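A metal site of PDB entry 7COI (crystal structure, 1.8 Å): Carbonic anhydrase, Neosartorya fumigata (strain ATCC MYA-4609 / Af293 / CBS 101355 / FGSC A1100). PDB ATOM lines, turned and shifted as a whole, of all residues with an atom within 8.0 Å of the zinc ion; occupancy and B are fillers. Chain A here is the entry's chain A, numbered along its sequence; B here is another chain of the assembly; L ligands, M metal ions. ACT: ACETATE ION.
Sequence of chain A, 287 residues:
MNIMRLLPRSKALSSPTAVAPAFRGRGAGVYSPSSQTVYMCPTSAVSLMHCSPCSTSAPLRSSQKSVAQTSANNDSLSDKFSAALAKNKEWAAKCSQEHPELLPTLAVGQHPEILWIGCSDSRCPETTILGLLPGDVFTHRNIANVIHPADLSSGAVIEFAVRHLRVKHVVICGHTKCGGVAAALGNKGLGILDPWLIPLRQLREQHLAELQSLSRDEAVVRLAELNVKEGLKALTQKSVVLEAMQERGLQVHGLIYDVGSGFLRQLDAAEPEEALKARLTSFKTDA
The backbone NH of Ala 144 sits close to the side-chain sulfur of Cys 119, at 3.3 Å. The side-chain sulfur of Cys 119 lies close to the backbone carbonyl oxygen of Asn 142 (3.7 Å). The side-chain sulfur (SG) of Cys 119 lies close to the backbone NH (N) of Asp 121, at 3.5 Å. SG of Cys 178 lies close to N of Val 181. The side-chain carboxylate (OD2) of Asp 121 is in hydrogen-bond range of the side-chain amide nitrogen (NE2) of Gln 110 of chain B (3.2 Å). The side-chain carboxylate (OD2) of Asp 121 lies within salt-bridge range of the guanidinium group (NH2) of Arg 123 (2.8 Å). The backbone NH of Gly 180 sits close to the side-chain sulfur of Cys 178 (3.7 Å).
Asp 121 touches the zinc ion (CB to ZN, 3.9 Å). Within 4 Å of the zinc ion: Cys 119, Asp 121, His 175 and Cys 178.
The zinc ion is bound by an oxygen (OXT) of the ligand, a ring nitrogen (NE2) of His 175, the side-chain sulfur (SG) of Cys 178 and the side-chain sulfur (SG) of Cys 119.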
ATOM      1  N   GLY A 118      -6.415 -31.173   4.446  1.00  0.00           N
ATOM      2  CA  GLY A 118      -6.595 -29.896   3.751  1.00  0.00           C
ATOM      3  C   GLY A 118      -6.352 -28.689   4.643  1.00  0.00           C
ATOM      4  O   GLY A 118      -5.879 -28.815   5.790  1.00  0.00           O
ATOM      5  N   CYS A 119      -6.647 -27.531   4.084  1.00  0.00           N
ATOM      6  CA  CYS A 119      -6.436 -26.253   4.781  1.00  0.00           C
ATOM      7  C   CYS A 119      -7.627 -25.989   5.708  1.00  0.00           C
ATOM      8  O   CYS A 119      -8.763 -26.346   5.361  1.00  0.00           O
ATOM      9  CB  CYS A 119      -6.180 -25.111   3.801  1.00  0.00           C
ATOM     10  SG  CYS A 119      -5.695 -23.665   4.695  1.00  0.00           S
ATOM     11  N   SER A 120      -7.358 -25.312   6.837  1.00  0.00           N
ATOM     12  CA  SER A 120      -8.401 -24.783   7.751  1.00  0.00           C
ATOM     13  C   SER A 120      -9.298 -23.721   7.089  1.00  0.00           C
ATOM     14  O   SER A 120     -10.380 -23.459   7.634  1.00  0.00           O
ATOM     15  CB  SER A 120      -7.739 -24.198   8.952  1.00  0.00           C
ATOM     16  OG  SER A 120      -7.002 -25.184   9.635  1.00  0.00           O
ATOM     17  N   ASP A 121      -8.839 -23.107   6.007  1.00  0.00           N
ATOM     18  CA  ASP A 121      -9.615 -22.086   5.238  1.00  0.00           C
ATOM     19  C   ASP A 121     -11.095 -22.472   5.236  1.00  0.00           C
ATOM     20  O   ASP A 121     -11.455 -23.632   4.875  1.00  0.00           O
ATOM     21  CB  ASP A 121      -9.031 -21.942   3.817  1.00  0.00           C
ATOM     22  CG  ASP A 121      -9.624 -20.743   3.066  1.00  0.00           C
ATOM     23  OD1 ASP A 121     -10.869 -20.654   2.935  1.00  0.00           O
ATOM     24  OD2 ASP A 121      -8.824 -19.867   2.691  1.00  0.00           O
ATOM     25  N   SER A 122     -11.957 -21.554   5.685  1.00  0.00           N
ATOM     26  CA  SER A 122     -13.396 -21.780   5.878  1.00  0.00           C
ATOM     27  C   SER A 122     -14.073 -22.140   4.542  1.00  0.00           C
ATOM     28  O   SER A 122     -15.189 -22.701   4.589  1.00  0.00           O
ATOM     29  CB  SER A 122     -14.046 -20.597   6.502  1.00  0.00           C
ATOM     30  OG  SER A 122     -13.977 -19.459   5.608  1.00  0.00           O
ATOM     31  N   ARG A 123     -13.438 -21.842   3.410  1.00  0.00           N
ATOM     32  CA  ARG A 123     -14.038 -22.099   2.087  1.00  0.00           C
ATOM     33  C   ARG A 123     -13.802 -23.541   1.634  1.00  0.00           C
ATOM     34  O   ARG A 123     -14.329 -23.865   0.560  1.00  0.00           O
ATOM     35  CB  ARG A 123     -13.491 -21.078   1.074  1.00  0.00           C
ATOM     36  CG  ARG A 123     -13.817 -19.651   1.483  1.00  0.00           C
ATOM     37  CD  ARG A 123     -13.035 -18.625   0.651  1.00  0.00           C
ATOM     38  NE  ARG A 123     -11.616 -18.670   0.944  1.00  0.00           N
ATOM     39  CZ  ARG A 123     -10.718 -17.783   0.506  1.00  0.00           C
ATOM     40  NH1 ARG A 123     -11.094 -16.799  -0.324  1.00  0.00           N
ATOM     41  NH2 ARG A 123      -9.443 -17.913   0.831  1.00  0.00           N
ATOM     42  N   CYS A 124     -13.096 -24.374   2.410  1.00  0.00           N
ATOM     43  CA  CYS A 124     -12.732 -25.760   1.984  1.00  0.00           C
ATOM     44  C   CYS A 124     -13.287 -26.803   2.950  1.00  0.00           C
ATOM     45  O   CYS A 124     -12.548 -27.668   3.409  1.00  0.00           O
ATOM     46  CB  CYS A 124     -11.220 -25.889   1.869  1.00  0.00           C
ATOM     47  SG  CYS A 124     -10.402 -24.521   1.013  1.00  0.00           S
ATOM     48  N   ASN A 142      -5.369 -27.965   8.736  1.00  0.00           N
ATOM     49  CA  ASN A 142      -4.358 -27.147   9.445  1.00  0.00           C
ATOM     50  C   ASN A 142      -4.040 -25.960   8.539  1.00  0.00           C
ATOM     51  O   ASN A 142      -4.606 -25.867   7.403  1.00  0.00           O
ATOM     52  CB  ASN A 142      -3.150 -27.986   9.876  1.00  0.00           C
ATOM     53  CG  ASN A 142      -2.308 -28.463   8.706  1.00  0.00           C
ATOM     54  OD1 ASN A 142      -2.408 -27.890   7.610  1.00  0.00           O
ATOM     55  ND2 ASN A 142      -1.484 -29.495   8.921  1.00  0.00           N
ATOM     56  N   ILE A 143      -3.159 -25.078   8.982  1.00  0.00           N
ATOM     57  CA  ILE A 143      -2.782 -23.896   8.160  1.00  0.00           C
ATOM     58  C   ILE A 143      -2.003 -24.358   6.915  1.00  0.00           C
ATOM     59  O   ILE A 143      -0.877 -24.902   7.043  1.00  0.00           O
ATOM     60  CB  ILE A 143      -2.002 -22.853   8.952  1.00  0.00           C
ATOM     61  CG1 ILE A 143      -2.829 -22.286  10.104  1.00  0.00           C
ATOM     62  CG2 ILE A 143      -1.537 -21.752   8.007  1.00  0.00           C
ATOM     63  CD1 ILE A 143      -4.155 -21.650   9.710  1.00  0.00           C
ATOM     64  N   ALA A 144      -2.601 -24.148   5.739  1.00  0.00           N
ATOM     65  CA  ALA A 144      -1.997 -24.400   4.414  1.00  0.00           C
ATOM     66  C   ALA A 144      -1.690 -25.879   4.208  1.00  0.00           C
ATOM     67  O   ALA A 144      -0.809 -26.201   3.376  1.00  0.00           O
ATOM     68  CB  ALA A 144      -0.731 -23.588   4.257  1.00  0.00           C
ATOM     69  N   ASN A 145      -2.437 -26.792   4.843  1.00  0.00           N
ATOM     70  CA  ASN A 145      -2.347 -28.244   4.531  1.00  0.00           C
ATOM     71  C   ASN A 145      -0.860 -28.640   4.520  1.00  0.00           C
ATOM     72  O   ASN A 145      -0.459 -29.431   3.654  1.00  0.00           O
ATOM     73  CB  ASN A 145      -3.122 -28.596   3.236  1.00  0.00           C
ATOM     74  CG  ASN A 145      -2.830 -27.754   2.013  1.00  0.00           C
ATOM     75  OD1 ASN A 145      -3.434 -26.702   1.827  1.00  0.00           O
ATOM     76  ND2 ASN A 145      -1.936 -28.216   1.146  1.00  0.00           N
ATOM     77  N   CYS A 173      -5.231 -31.847  -0.147  1.00  0.00           N
ATOM     78  CA  CYS A 173      -5.917 -30.823  -0.940  1.00  0.00           C
ATOM     79  C   CYS A 173      -5.394 -29.465  -0.526  1.00  0.00           C
ATOM     80  O   CYS A 173      -5.634 -29.047   0.605  1.00  0.00           O
ATOM     81  CB  CYS A 173      -7.432 -30.953  -0.764  1.00  0.00           C
ATOM     82  SG  CYS A 173      -8.318 -29.787  -1.824  1.00  0.00           S
ATOM     83  N   GLY A 174      -4.685 -28.805  -1.441  1.00  0.00           N
ATOM     84  CA  GLY A 174      -4.374 -27.368  -1.355  1.00  0.00           C
ATOM     85  C   GLY A 174      -5.454 -26.554  -2.024  1.00  0.00           C
ATOM     86  O   GLY A 174      -6.441 -27.132  -2.537  1.00  0.00           O
ATOM     87  N   HIS A 175      -5.355 -25.227  -1.994  1.00  0.00           N
ATOM     88  CA  HIS A 175      -6.460 -24.431  -2.585  1.00  0.00           C
ATOM     89  C   HIS A 175      -5.883 -23.107  -3.079  1.00  0.00           C
ATOM     90  O   HIS A 175      -4.775 -22.699  -2.681  1.00  0.00           O
ATOM     91  CB  HIS A 175      -7.668 -24.297  -1.631  1.00  0.00           C
ATOM     92  CG  HIS A 175      -7.298 -23.445  -0.479  1.00  0.00           C
ATOM     93  ND1 HIS A 175      -7.704 -22.114  -0.395  1.00  0.00           N
ATOM     94  CD2 HIS A 175      -6.512 -23.692   0.590  1.00  0.00           C
ATOM     95  CE1 HIS A 175      -7.211 -21.571   0.679  1.00  0.00           C
ATOM     96  NE2 HIS A 175      -6.516 -22.532   1.285  1.00  0.00           N
ATOM     97  N   THR A 176      -6.613 -22.501  -4.006  1.00  0.00           N
ATOM     98  CA  THR A 176      -6.297 -21.159  -4.538  1.00  0.00           C
ATOM     99  C   THR A 176      -6.605 -20.144  -3.432  1.00  0.00           C
ATOM    100  O   THR A 176      -7.513 -20.394  -2.589  1.00  0.00           O
ATOM    101  CB  THR A 176      -7.054 -20.911  -5.849  1.00  0.00           C
ATOM    102  OG1 THR A 176      -8.454 -20.861  -5.565  1.00  0.00           O
ATOM    103  CG2 THR A 176      -6.770 -21.983  -6.877  1.00  0.00           C
ATOM    104  N   LYS A 177      -5.899 -19.017  -3.457  1.00  0.00           N
ATOM    105  CA  LYS A 177      -6.100 -17.904  -2.490  1.00  0.00           C
ATOM    106  C   LYS A 177      -5.790 -18.375  -1.059  1.00  0.00           C
ATOM    107  O   LYS A 177      -6.494 -17.953  -0.143  1.00  0.00           O
ATOM    108  CB  LYS A 177      -7.521 -17.370  -2.584  1.00  0.00           C
ATOM    109  CG  LYS A 177      -7.978 -17.054  -4.016  1.00  0.00           C
ATOM    110  CD  LYS A 177      -7.275 -15.870  -4.590  1.00  0.00           C
ATOM    111  CE  LYS A 177      -7.778 -14.563  -4.009  1.00  0.00           C
ATOM    112  NZ  LYS A 177      -6.692 -13.597  -3.678  1.00  0.00           N
ATOM    113  N   CYS A 178      -4.811 -19.252  -0.884  1.00  0.00           N
ATOM    114  CA  CYS A 178      -4.389 -19.773   0.459  1.00  0.00           C
ATOM    115  C   CYS A 178      -3.575 -18.702   1.177  1.00  0.00           C
ATOM    116  O   CYS A 178      -2.467 -18.419   0.721  1.00  0.00           O
ATOM    117  CB  CYS A 178      -3.617 -21.080   0.353  1.00  0.00           C
ATOM    118  SG  CYS A 178      -3.212 -21.750   1.980  1.00  0.00           S
ATOM    119  N   GLY A 179      -4.092 -18.185   2.293  1.00  0.00           N
ATOM    120  CA  GLY A 179      -3.408 -17.183   3.150  1.00  0.00           C
ATOM    121  C   GLY A 179      -2.108 -17.691   3.741  1.00  0.00           C
ATOM    122  O   GLY A 179      -1.214 -16.879   3.937  1.00  0.00           O
ATOM    123  N   GLY A 180      -1.959 -18.976   4.021  1.00  0.00           N
ATOM    124  CA  GLY A 180      -0.707 -19.529   4.556  1.00  0.00           C
ATOM    125  C   GLY A 180       0.344 -19.563   3.478  1.00  0.00           C
ATOM    126  O   GLY A 180       1.486 -19.171   3.715  1.00  0.00           O
ATOM    127  N   VAL A 181      -0.029 -19.997   2.282  1.00  0.00           N
ATOM    128  CA  VAL A 181       0.911 -19.979   1.126  1.00  0.00           C
ATOM    129  C   VAL A 181       1.316 -18.512   0.879  1.00  0.00           C
ATOM    130  O   VAL A 181       2.526 -18.233   0.718  1.00  0.00           O
ATOM    131  CB  VAL A 181       0.270 -20.643  -0.085  1.00  0.00           C
ATOM    132  CG1 VAL A 181       1.121 -20.432  -1.332  1.00  0.00           C
ATOM    133  CG2 VAL A 181       0.045 -22.133   0.184  1.00  0.00           C
ATOM    134  N   ALA A 182       0.368 -17.587   0.840  1.00  0.00           N
ATOM    135  CA  ALA A 182       0.675 -16.144   0.590  1.00  0.00           C
ATOM    136  C   ALA A 182       1.615 -15.603   1.683  1.00  0.00           C
ATOM    137  O   ALA A 182       2.579 -14.869   1.380  1.00  0.00           O
ATOM    138  CB  ALA A 182      -0.591 -15.344   0.488  1.00  0.00           C
ATOM    139  N   ALA A 224       1.310 -23.350  -3.801  1.00  0.00           N
ATOM    140  CA  ALA A 224       0.252 -24.239  -3.263  1.00  0.00           C
ATOM    141  C   ALA A 224       0.395 -25.630  -3.874  1.00  0.00           C
ATOM    142  O   ALA A 224       0.291 -26.607  -3.179  1.00  0.00           O
ATOM    143  CB  ALA A 224      -1.119 -23.649  -3.512  1.00  0.00           C
ATOM    144  N   VAL A 259     -11.361 -21.957  -4.979  1.00  0.00           N
ATOM    145  CA  VAL A 259     -12.393 -21.377  -4.071  1.00  0.00           C
ATOM    146  C   VAL A 259     -13.398 -20.556  -4.871  1.00  0.00           C
ATOM    147  O   VAL A 259     -14.490 -20.294  -4.330  1.00  0.00           O
ATOM    148  CB  VAL A 259     -11.758 -20.556  -2.934  1.00  0.00           C
ATOM    149  CG1 VAL A 259     -10.853 -21.429  -2.082  1.00  0.00           C
ATOM    150  CG2 VAL A 259     -11.002 -19.359  -3.482  1.00  0.00           C
ATOM    151  N   GLN B 110     -12.353 -14.705   2.587  1.00  0.00           N
ATOM    152  CA  GLN B 110     -13.195 -15.375   3.616  1.00  0.00           C
ATOM    153  C   GLN B 110     -13.382 -14.442   4.806  1.00  0.00           C
ATOM    154  O   GLN B 110     -12.426 -13.701   5.156  1.00  0.00           O
ATOM    155  CB  GLN B 110     -12.534 -16.685   4.035  1.00  0.00           C
ATOM    156  CG  GLN B 110     -11.244 -16.495   4.817  1.00  0.00           C
ATOM    157  CD  GLN B 110     -10.653 -17.807   5.269  1.00  0.00           C
ATOM    158  OE1 GLN B 110     -11.377 -18.686   5.737  1.00  0.00           O
ATOM    159  NE2 GLN B 110      -9.338 -17.953   5.146  1.00  0.00           N
ATOM    160  N   PHE B 138     -14.003 -21.636   9.964  1.00  0.00           N
ATOM    161  CA  PHE B 138     -12.539 -21.894   9.917  1.00  0.00           C
ATOM    162  C   PHE B 138     -12.271 -23.099  10.810  1.00  0.00           C
ATOM    163  O   PHE B 138     -12.786 -23.133  11.939  1.00  0.00           O
ATOM    164  CB  PHE B 138     -11.766 -20.656  10.333  1.00  0.00           C
ATOM    165  CG  PHE B 138     -10.300 -20.705  10.004  1.00  0.00           C
ATOM    166  CD1 PHE B 138      -9.889 -20.432   8.718  1.00  0.00           C
ATOM    167  CD2 PHE B 138      -9.334 -20.900  10.970  1.00  0.00           C
ATOM    168  CE1 PHE B 138      -8.532 -20.424   8.401  1.00  0.00           C
ATOM    169  CE2 PHE B 138      -7.976 -20.923  10.654  1.00  0.00           C
ATOM    170  CZ  PHE B 138      -7.569 -20.670   9.356  1.00  0.00           C
ATOM    171  N   PHE B 160      -3.923 -17.611  13.494  1.00  0.00           N
ATOM    172  CA  PHE B 160      -4.482 -17.145  12.186  1.00  0.00           C
ATOM    173  C   PHE B 160      -5.958 -16.762  12.358  1.00  0.00           C
ATOM    174  O   PHE B 160      -6.357 -15.662  11.950  1.00  0.00           O
ATOM    175  CB  PHE B 160      -4.267 -18.202  11.113  1.00  0.00           C
ATOM    176  CG  PHE B 160      -4.481 -17.645   9.727  1.00  0.00           C
ATOM    177  CD1 PHE B 160      -5.748 -17.555   9.184  1.00  0.00           C
ATOM    178  CD2 PHE B 160      -3.396 -17.174   9.000  1.00  0.00           C
ATOM    179  CE1 PHE B 160      -5.934 -17.002   7.923  1.00  0.00           C
ATOM    180  CE2 PHE B 160      -3.591 -16.622   7.734  1.00  0.00           C
ATOM    181  CZ  PHE B 160      -4.863 -16.510   7.222  1.00  0.00           C
HETATM  182  C   ACT L   1      -6.040 -20.028   5.045  1.00  0.00           C
HETATM  183  O   ACT L   1      -7.103 -19.522   5.406  1.00  0.00           O
HETATM  184  OXT ACT L   1      -5.887 -20.350   3.625  1.00  0.00           O
HETATM  185  CH3 ACT L   1      -4.886 -20.356   6.006  1.00  0.00           C
HETATM  186 ZN    ZN M   1      -5.273 -22.126   2.985  1.00  0.00          ZN
